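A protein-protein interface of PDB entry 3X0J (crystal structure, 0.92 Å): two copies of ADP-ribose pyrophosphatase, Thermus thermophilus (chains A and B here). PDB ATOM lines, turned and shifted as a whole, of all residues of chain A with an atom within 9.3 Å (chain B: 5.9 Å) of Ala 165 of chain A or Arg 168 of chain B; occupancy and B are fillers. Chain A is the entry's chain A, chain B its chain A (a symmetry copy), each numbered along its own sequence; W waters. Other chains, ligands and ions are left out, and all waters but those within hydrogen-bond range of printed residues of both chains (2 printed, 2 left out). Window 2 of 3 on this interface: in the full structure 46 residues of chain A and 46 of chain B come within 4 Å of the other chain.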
ATOM      1  N   MET A  47      32.892  12.907 -28.244  1.00  0.00           N
ATOM      2  CA  MET A  47      31.886  11.911 -27.891  1.00  0.00           C
ATOM      3  C   MET A  47      32.388  10.536 -28.262  1.00  0.00           C
ATOM      4  O   MET A  47      33.098  10.327 -29.252  1.00  0.00           O
ATOM      5  CB  MET A  47      30.574  12.275 -28.605  1.00  0.00           C
ATOM      6  CG  MET A  47      29.436  11.250 -28.358  1.00  0.00           C
ATOM      7  SD  MET A  47      27.821  12.016 -28.697  1.00  0.00           S
ATOM      8  CE  MET A  47      27.753  13.137 -27.412  1.00  0.00           C
ATOM      9  N   PHE A  97      16.428   9.398 -20.731  1.00  0.00           N
ATOM     10  CA  PHE A  97      15.141   9.352 -21.407  1.00  0.00           C
ATOM     11  C   PHE A  97      15.096   8.063 -22.223  1.00  0.00           C
ATOM     12  O   PHE A  97      16.135   7.380 -22.350  1.00  0.00           O
ATOM     13  CB  PHE A  97      14.847  10.601 -22.250  1.00  0.00           C
ATOM     14  CG  PHE A  97      16.039  11.134 -23.022  1.00  0.00           C
ATOM     15  CD1 PHE A  97      16.478  12.441 -22.784  1.00  0.00           C
ATOM     16  CD2 PHE A  97      16.718  10.378 -23.954  1.00  0.00           C
ATOM     17  CE1 PHE A  97      17.579  12.968 -23.459  1.00  0.00           C
ATOM     18  CE2 PHE A  97      17.832  10.836 -24.628  1.00  0.00           C
ATOM     19  CZ  PHE A  97      18.292  12.161 -24.380  1.00  0.00           C
ATOM     20  N   PRO A 138      31.380  15.970 -31.414  1.00  0.00           N
ATOM     21  CA  PRO A 138      30.065  15.879 -32.006  1.00  0.00           C
ATOM     22  C   PRO A 138      29.873  16.869 -33.143  1.00  0.00           C
ATOM     23  O   PRO A 138      29.057  16.605 -34.077  1.00  0.00           O
ATOM     24  CB  PRO A 138      29.085  16.192 -30.871  1.00  0.00           C
ATOM     25  CG  PRO A 138      29.855  15.768 -29.674  1.00  0.00           C
ATOM     26  CD  PRO A 138      31.294  16.107 -29.933  1.00  0.00           C
ATOM     27  N   GLU A 139      30.498  18.042 -33.075  1.00  0.00           N
ATOM     28  CA  GLU A 139      30.363  19.019 -34.153  1.00  0.00           C
ATOM     29  C   GLU A 139      30.910  18.443 -35.424  1.00  0.00           C
ATOM     30  O   GLU A 139      30.365  18.703 -36.505  1.00  0.00           O
ATOM     31  CB  GLU A 139      31.187  20.267 -33.781  1.00  0.00           C
ATOM     32  CG  GLU A 139      30.686  20.995 -32.541  1.00  0.00           C
ATOM     33  CD  GLU A 139      31.209  20.580 -31.206  1.00  0.00           C
ATOM     34  OE1 GLU A 139      31.782  19.459 -31.077  1.00  0.00           O
ATOM     35  OE2 GLU A 139      31.009  21.347 -30.227  1.00  0.00           O
ATOM     36  N   LEU A 157      22.661   9.891 -33.555  1.00  0.00           N
ATOM     37  CA  LEU A 157      22.053  11.201 -33.716  1.00  0.00           C
ATOM     38  C   LEU A 157      21.551  11.754 -32.399  1.00  0.00           C
ATOM     39  O   LEU A 157      21.741  12.949 -32.107  1.00  0.00           O
ATOM     40  CB  LEU A 157      20.930  11.113 -34.760  1.00  0.00           C
ATOM     41  CG  LEU A 157      20.164  12.412 -34.977  1.00  0.00           C
ATOM     42  CD1 LEU A 157      21.048  13.506 -35.537  1.00  0.00           C
ATOM     43  CD2 LEU A 157      18.968  12.141 -35.917  1.00  0.00           C
ATOM     44  N   VAL A 158      20.898  10.919 -31.607  1.00  0.00           N
ATOM     45  CA  VAL A 158      20.455  11.362 -30.270  1.00  0.00           C
ATOM     46  C   VAL A 158      21.643  11.840 -29.452  1.00  0.00           C
ATOM     47  O   VAL A 158      21.548  12.883 -28.788  1.00  0.00           O
ATOM     48  CB  VAL A 158      19.675  10.215 -29.584  1.00  0.00           C
ATOM     49  CG1 VAL A 158      19.555  10.451 -28.070  1.00  0.00           C
ATOM     50  CG2 VAL A 158      18.300  10.057 -30.242  1.00  0.00           C
ATOM     51  N   GLY A 159      22.774  11.127 -29.489  1.00  0.00           N
ATOM     52  CA  GLY A 159      23.932  11.590 -28.742  1.00  0.00           C
ATOM     53  C   GLY A 159      24.391  12.970 -29.214  1.00  0.00           C
ATOM     54  O   GLY A 159      24.672  13.864 -28.404  1.00  0.00           O
ATOM     55  N   VAL A 160      24.494  13.161 -30.529  1.00  0.00           N
ATOM     56  CA  VAL A 160      24.924  14.434 -31.062  1.00  0.00           C
ATOM     57  C   VAL A 160      23.991  15.551 -30.690  1.00  0.00           C
ATOM     58  O   VAL A 160      24.417  16.661 -30.299  1.00  0.00           O
ATOM     59  CB  VAL A 160      25.075  14.314 -32.606  1.00  0.00           C
ATOM     60  CG1 VAL A 160      25.187  15.662 -33.273  1.00  0.00           C
ATOM     61  CG2 VAL A 160      26.266  13.443 -32.977  1.00  0.00           C
ATOM     62  N   LEU A 161      22.685  15.307 -30.812  1.00  0.00           N
ATOM     63  CA  LEU A 161      21.720  16.378 -30.489  1.00  0.00           C
ATOM     64  C   LEU A 161      21.715  16.674 -28.994  1.00  0.00           C
ATOM     65  O   LEU A 161      21.621  17.837 -28.588  1.00  0.00           O
ATOM     66  CB  LEU A 161      20.346  16.017 -31.004  1.00  0.00           C
ATOM     67  CG  LEU A 161      20.211  15.895 -32.510  1.00  0.00           C
ATOM     68  CD1 LEU A 161      18.810  15.451 -32.875  1.00  0.00           C
ATOM     69  CD2 LEU A 161      20.561  17.202 -33.236  1.00  0.00           C
ATOM     70  N   TYR A 162      21.772  15.622 -28.160  1.00  0.00           N
ATOM     71  CA  TYR A 162      21.808  15.839 -26.719  1.00  0.00           C
ATOM     72  C   TYR A 162      23.025  16.695 -26.350  1.00  0.00           C
ATOM     73  O   TYR A 162      22.908  17.619 -25.524  1.00  0.00           O
ATOM     74  CB  TYR A 162      21.845  14.468 -25.999  1.00  0.00           C
ATOM     75  CG  TYR A 162      21.859  14.666 -24.498  1.00  0.00           C
ATOM     76  CD1 TYR A 162      20.668  14.859 -23.834  1.00  0.00           C
ATOM     77  CD2 TYR A 162      23.045  14.711 -23.795  1.00  0.00           C
ATOM     78  CE1 TYR A 162      20.662  15.057 -22.449  1.00  0.00           C
ATOM     79  CE2 TYR A 162      23.021  14.944 -22.442  1.00  0.00           C
ATOM     80  CZ  TYR A 162      21.851  15.121 -21.776  1.00  0.00           C
ATOM     81  OH  TYR A 162      21.860  15.370 -20.388  1.00  0.00           O
ATOM     82  N   TYR A 163      24.180  16.370 -26.918  1.00  0.00           N
ATOM     83  CA  TYR A 163      25.362  17.185 -26.634  1.00  0.00           C
ATOM     84  C   TYR A 163      25.113  18.657 -26.937  1.00  0.00           C
ATOM     85  O   TYR A 163      25.440  19.540 -26.191  1.00  0.00           O
ATOM     86  CB  TYR A 163      26.569  16.654 -27.459  1.00  0.00           C
ATOM     87  CG  TYR A 163      27.696  17.657 -27.565  1.00  0.00           C
ATOM     88  CD1 TYR A 163      28.664  17.748 -26.571  1.00  0.00           C
ATOM     89  CD2 TYR A 163      27.804  18.503 -28.667  1.00  0.00           C
ATOM     90  CE1 TYR A 163      29.711  18.659 -26.672  1.00  0.00           C
ATOM     91  CE2 TYR A 163      28.814  19.443 -28.779  1.00  0.00           C
ATOM     92  CZ  TYR A 163      29.759  19.484 -27.771  1.00  0.00           C
ATOM     93  OH  TYR A 163      30.793  20.413 -27.835  1.00  0.00           O
ATOM     94  N   HIS A 164      24.599  18.897 -28.168  1.00  0.00           N
ATOM     95  CA  HIS A 164      24.453  20.304 -28.580  1.00  0.00           C
ATOM     96  C   HIS A 164      23.430  21.002 -27.689  1.00  0.00           C
ATOM     97  O   HIS A 164      23.564  22.200 -27.466  1.00  0.00           O
ATOM     98  CB  HIS A 164      24.071  20.384 -30.058  1.00  0.00           C
ATOM     99  CG  HIS A 164      25.178  20.173 -31.030  1.00  0.00           C
ATOM    100  ND1 HIS A 164      25.568  18.932 -31.466  1.00  0.00           N
ATOM    101  CD2 HIS A 164      25.992  21.086 -31.642  1.00  0.00           C
ATOM    102  CE1 HIS A 164      26.637  19.099 -32.334  1.00  0.00           C
ATOM    103  NE2 HIS A 164      26.886  20.400 -32.483  1.00  0.00           N
ATOM    104  N   ALA A 165      22.414  20.276 -27.221  1.00  0.00           N
ATOM    105  CA  ALA A 165      21.382  20.870 -26.403  1.00  0.00           C
ATOM    106  C   ALA A 165      21.850  21.151 -24.958  1.00  0.00           C
ATOM    107  O   ALA A 165      21.489  22.187 -24.400  1.00  0.00           O
ATOM    108  CB  ALA A 165      20.170  19.967 -26.336  1.00  0.00           C
ATOM    109  N   PHE A 166      22.615  20.240 -24.379  1.00  0.00           N
ATOM    110  CA  PHE A 166      22.785  20.260 -22.928  1.00  0.00           C
ATOM    111  C   PHE A 166      24.220  20.144 -22.434  1.00  0.00           C
ATOM    112  O   PHE A 166      24.432  20.379 -21.244  1.00  0.00           O
ATOM    113  CB  PHE A 166      21.993  19.120 -22.305  1.00  0.00           C
ATOM    114  CG  PHE A 166      20.522  19.225 -22.565  1.00  0.00           C
ATOM    115  CD1 PHE A 166      19.847  18.258 -23.282  1.00  0.00           C
ATOM    116  CD2 PHE A 166      19.814  20.301 -22.054  1.00  0.00           C
ATOM    117  CE1 PHE A 166      18.492  18.391 -23.514  1.00  0.00           C
ATOM    118  CE2 PHE A 166      18.431  20.434 -22.334  1.00  0.00           C
ATOM    119  CZ  PHE A 166      17.751  19.456 -23.033  1.00  0.00           C
ATOM    120  N   LEU A 167      25.202  19.838 -23.300  1.00  0.00           N
ATOM    121  CA  LEU A 167      26.558  19.570 -22.799  1.00  0.00           C
ATOM    122  C   LEU A 167      27.649  20.547 -23.242  1.00  0.00           C
ATOM    123  O   LEU A 167      28.838  20.352 -22.993  1.00  0.00           O
ATOM    124  CB  LEU A 167      26.997  18.168 -23.213  1.00  0.00           C
ATOM    125  CG  LEU A 167      26.192  16.998 -22.686  1.00  0.00           C
ATOM    126  CD1 LEU A 167      26.689  15.658 -23.130  1.00  0.00           C
ATOM    127  CD2 LEU A 167      26.163  17.002 -21.171  1.00  0.00           C
ATOM    128  N   ARG A 168      27.227  21.641 -23.819  1.00  0.00           N
ATOM    129  CA  ARG A 168      28.260  22.631 -24.247  1.00  0.00           C
ATOM    130  C   ARG A 168      28.546  23.664 -23.200  1.00  0.00           C
ATOM    131  O   ARG A 168      28.038  23.685 -22.109  1.00  0.00           O
ATOM    132  CB  ARG A 168      27.761  23.293 -25.558  1.00  0.00           C
ATOM    133  CG  ARG A 168      27.766  22.263 -26.708  1.00  0.00           C
ATOM    134  CD  ARG A 168      27.769  22.977 -28.022  1.00  0.00           C
ATOM    135  NE  ARG A 168      26.345  23.443 -28.160  1.00  0.00           N
ATOM    136  CZ  ARG A 168      25.939  24.115 -29.219  1.00  0.00           C
ATOM    137  NH1 ARG A 168      26.887  24.394 -30.164  1.00  0.00           N
ATOM    138  NH2 ARG A 168      24.703  24.520 -29.323  1.00  0.00           N
ATOM    139  N   GLU B 139       9.808  21.916 -23.999  1.00  0.00           N
ATOM    140  CA  GLU B 139      10.242  21.804 -22.608  1.00  0.00           C
ATOM    141  C   GLU B 139       9.226  21.026 -21.827  1.00  0.00           C
ATOM    142  O   GLU B 139       9.594  20.254 -20.930  1.00  0.00           O
ATOM    143  CB  GLU B 139      10.341  23.223 -22.015  1.00  0.00           C
ATOM    144  CG  GLU B 139      11.396  24.099 -22.675  1.00  0.00           C
ATOM    145  CD  GLU B 139      11.012  24.911 -23.866  1.00  0.00           C
ATOM    146  OE1 GLU B 139       9.954  24.632 -24.502  1.00  0.00           O
ATOM    147  OE2 GLU B 139      11.793  25.827 -24.237  1.00  0.00           O
ATOM    148  N   LEU B 161      15.065  17.264 -28.934  1.00  0.00           N
ATOM    149  CA  LEU B 161      16.503  17.559 -28.762  1.00  0.00           C
ATOM    150  C   LEU B 161      16.970  18.599 -29.774  1.00  0.00           C
ATOM    151  O   LEU B 161      17.770  19.478 -29.442  1.00  0.00           O
ATOM    152  CB  LEU B 161      17.311  16.284 -28.839  1.00  0.00           C
ATOM    153  CG  LEU B 161      17.051  15.265 -27.746  1.00  0.00           C
ATOM    154  CD1 LEU B 161      17.866  14.013 -27.994  1.00  0.00           C
ATOM    155  CD2 LEU B 161      17.346  15.822 -26.345  1.00  0.00           C
ATOM    156  N   TYR B 163      15.224  20.980 -31.099  1.00  0.00           N
ATOM    157  CA  TYR B 163      14.776  22.287 -30.615  1.00  0.00           C
ATOM    158  C   TYR B 163      15.731  22.856 -29.574  1.00  0.00           C
ATOM    159  O   TYR B 163      16.105  23.998 -29.588  1.00  0.00           O
ATOM    160  CB  TYR B 163      13.341  22.160 -30.029  1.00  0.00           C
ATOM    161  CG  TYR B 163      12.963  23.322 -29.139  1.00  0.00           C
ATOM    162  CD1 TYR B 163      12.429  24.488 -29.679  1.00  0.00           C
ATOM    163  CD2 TYR B 163      13.124  23.252 -27.757  1.00  0.00           C
ATOM    164  CE1 TYR B 163      12.067  25.555 -28.862  1.00  0.00           C
ATOM    165  CE2 TYR B 163      12.804  24.310 -26.923  1.00  0.00           C
ATOM    166  CZ  TYR B 163      12.265  25.440 -27.506  1.00  0.00           C
ATOM    167  OH  TYR B 163      11.929  26.532 -26.712  1.00  0.00           O
ATOM    168  N   HIS B 164      16.033  22.004 -28.565  1.00  0.00           N
ATOM    169  CA  HIS B 164      16.847  22.529 -27.454  1.00  0.00           C
ATOM    170  C   HIS B 164      18.239  22.896 -27.960  1.00  0.00           C
ATOM    171  O   HIS B 164      18.837  23.817 -27.417  1.00  0.00           O
ATOM    172  CB  HIS B 164      16.904  21.510 -26.315  1.00  0.00           C
ATOM    173  CG  HIS B 164      15.698  21.433 -25.448  1.00  0.00           C
ATOM    174  ND1 HIS B 164      14.609  20.653 -25.742  1.00  0.00           N
ATOM    175  CD2 HIS B 164      15.423  22.077 -24.273  1.00  0.00           C
ATOM    176  CE1 HIS B 164      13.664  20.843 -24.746  1.00  0.00           C
ATOM    177  NE2 HIS B 164      14.152  21.674 -23.826  1.00  0.00           N
ATOM    178  N   ALA B 165      18.753  22.169 -28.954  1.00  0.00           N
ATOM    179  CA  ALA B 165      20.079  22.427 -29.464  1.00  0.00           C
ATOM    180  C   ALA B 165      20.145  23.690 -30.349  1.00  0.00           C
ATOM    181  O   ALA B 165      21.122  24.435 -30.263  1.00  0.00           O
ATOM    182  CB  ALA B 165      20.573  21.255 -30.281  1.00  0.00           C
ATOM    183  N   PHE B 166      19.139  23.903 -31.182  1.00  0.00           N
ATOM    184  CA  PHE B 166      19.303  24.848 -32.283  1.00  0.00           C
ATOM    185  C   PHE B 166      18.177  25.858 -32.454  1.00  0.00           C
ATOM    186  O   PHE B 166      18.373  26.805 -33.216  1.00  0.00           O
ATOM    187  CB  PHE B 166      19.437  24.087 -33.594  1.00  0.00           C
ATOM    188  CG  PHE B 166      20.632  23.185 -33.621  1.00  0.00           C
ATOM    189  CD1 PHE B 166      20.499  21.817 -33.749  1.00  0.00           C
ATOM    190  CD2 PHE B 166      21.903  23.734 -33.545  1.00  0.00           C
ATOM    191  CE1 PHE B 166      21.622  21.013 -33.760  1.00  0.00           C
ATOM    192  CE2 PHE B 166      23.039  22.887 -33.523  1.00  0.00           C
ATOM    193  CZ  PHE B 166      22.907  21.521 -33.672  1.00  0.00           C
ATOM    194  N   LEU B 167      17.040  25.717 -31.749  1.00  0.00           N
ATOM    195  CA  LEU B 167      15.896  26.597 -32.029  1.00  0.00           C
ATOM    196  C   LEU B 167      15.466  27.529 -30.896  1.00  0.00           C
ATOM    197  O   LEU B 167      14.446  28.215 -30.967  1.00  0.00           O
ATOM    198  CB  LEU B 167      14.682  25.759 -32.424  1.00  0.00           C
ATOM    199  CG  LEU B 167      14.791  24.917 -33.680  1.00  0.00           C
ATOM    200  CD1 LEU B 167      13.559  24.132 -34.004  1.00  0.00           C
ATOM    201  CD2 LEU B 167      15.120  25.781 -34.881  1.00  0.00           C
ATOM    202  N   ARG B 168      16.296  27.618 -29.891  1.00  0.00           N
ATOM    203  CA  ARG B 168      15.923  28.535 -28.773  1.00  0.00           C
ATOM    204  C   ARG B 168      16.472  29.918 -28.946  1.00  0.00           C
ATOM    205  O   ARG B 168      17.114  30.281 -29.899  1.00  0.00           O
ATOM    206  CB  ARG B 168      16.431  27.898 -27.453  1.00  0.00           C
ATOM    207  CG  ARG B 168      15.627  26.617 -27.139  1.00  0.00           C
ATOM    208  CD  ARG B 168      15.756  26.287 -25.685  1.00  0.00           C
ATOM    209  NE  ARG B 168      17.137  25.699 -25.592  1.00  0.00           N
ATOM    210  CZ  ARG B 168      17.626  25.265 -24.448  1.00  0.00           C
ATOM    211  NH1 ARG B 168      16.825  25.410 -23.348  1.00  0.00           N
ATOM    212  NH2 ARG B 168      18.829  24.763 -24.379  1.00  0.00           N
HETATM  213  O   HOH W   1      23.331  26.612 -31.275  1.00  0.00           O
HETATM  214  O   HOH W   2      20.705  24.129 -21.899  1.00  0.00           O
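A ring nitrogen (ND1) of His 164 of chain A is in hydrogen-bond range of the backbone carbonyl oxygen (O) of Val 160 of chain A (2.8 Å). O of His 164 of chain A sits at hydrogen-bond distance from NE of Arg 168 of chain A, at 3.1 Å. The guanidinium group (NE) of Arg 168 of chain B is in hydrogen-bond range of the backbone carbonyl oxygen (O) of His 164 of chain B (3.1 Å).
Among the printed residues, merely in contact across the chains: His 164 of chain A with Ala 165 of chain B, Ala 165 of chain A with His 164 of chain B, Ala 165 of chain A with Ala 165 of chain B, Ala 165 of chain A with Arg 168 of chain B, Arg 168 of chain A with Ala 165 of chain B, Phe 166 of chain A with His 164 of chain B, His 164 of chain A with Phe 166 of chain B, Leu 161 of chain A with Leu 161 of chain B, Val 158 of chain A with Leu 161 of chain B, Ala 165 of chain A with Leu 161 of chain B, Leu 161 of chain A with Ala 165 of chain B, Leu 161 of chain A with Phe 166 of chain B and Phe 166 of chain A with Leu 161 of chain B.
Water W2 lies within hydrogen-bond range of NH2 of Arg 168 of chain B and O of Ala 165 of chain A. Water W1 bridges NH2 of Arg 168 of chain A (3.2 Å) and O of Ala 165 of chain B (3.3 Å).
Leu 161 of chain A touches its own counterpart, Leu 161 of chain B. Leu 161 of chain A touches Phe 166 of chain B, and with the chains exchanged Phe 166 of chain A touches Leu 161 of chain B. His 164 of chain A touches Ala 165 of chain B, and with the chains exchanged Ala 165 of chain A touches His 164 of chain B. His 164 of chain A touches Phe 166 of chain B, and with the chains exchanged Phe 166 of chain A touches His 164 of chain B. Positions printed for both chains: 139, 161, 163, 164, 165, 166, 167 and 168. Of the 13 pairs that touch across the chains among the printed residues, 12 have their exchanged pair printed and touching as well.
Hydrophobic or aromatic side chains of chain B that line the printed part of chain A: Leu 161, His 164, Ala 165 and Phe 166. Printed residues of chain A that touch a printed residue of chain B: Val 158, Leu 161, His 164, Ala 165, Phe 166 and Arg 168. Among the printed residues, 13 pairs touch across the chains. Among the printed residues, no Asp or Glu carboxylate lies within 4 Å of a Lys or Arg side-chain nitrogen of the other chain.
Ala 165 of chain A touches just these residues of chain B: Leu 161 (3.96 Å), His 164 (3.6 Å), Ala 165 (3.7 Å) and Arg 168 (3.7 Å). Printed residues of chain A within 4 Å of Ala 165 of chain B: Leu 161 (3.96 Å), His 164 (3.6 Å), Ala 165 (3.7 Å) and Arg 168 (3.7 Å). Of the printed residues of chain B, Phe 166 of chain A touches Leu 161 (3.99 Å) and His 164 (3.7 Å). Of the printed residues of chain B, Leu 161 of chain A touches Leu 161 (3.7 Å), Ala 165 (3.96 Å) and Phe 166 (3.99 Å). Printed residues of chain A within 4 Å of Leu 161 of chain B: Val 158 (3.9 Å), Leu 161 (3.7 Å), Ala 165 (3.96 Å) and Phe 166 (3.99 Å). Printed residues of chain A within 4 Å of His 164 of chain B: Ala 165 and Phe 166. Met 47 of chain A touches none of the printed residues of chain B. Pro 138 of chain A touches none of the printed residues of chain B. The nearest printed residue of chain B that does not touch Ala 165 of chain A is Phe 166 of chain B (6.1 Å). The nearest residue of chain A that does not touch Arg 168 of chain B is Phe 166 of chain A (4.8 Å). The nearest printed residue of chain A that does not touch His 164 of chain B is His 164 of chain A (5.0 Å).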
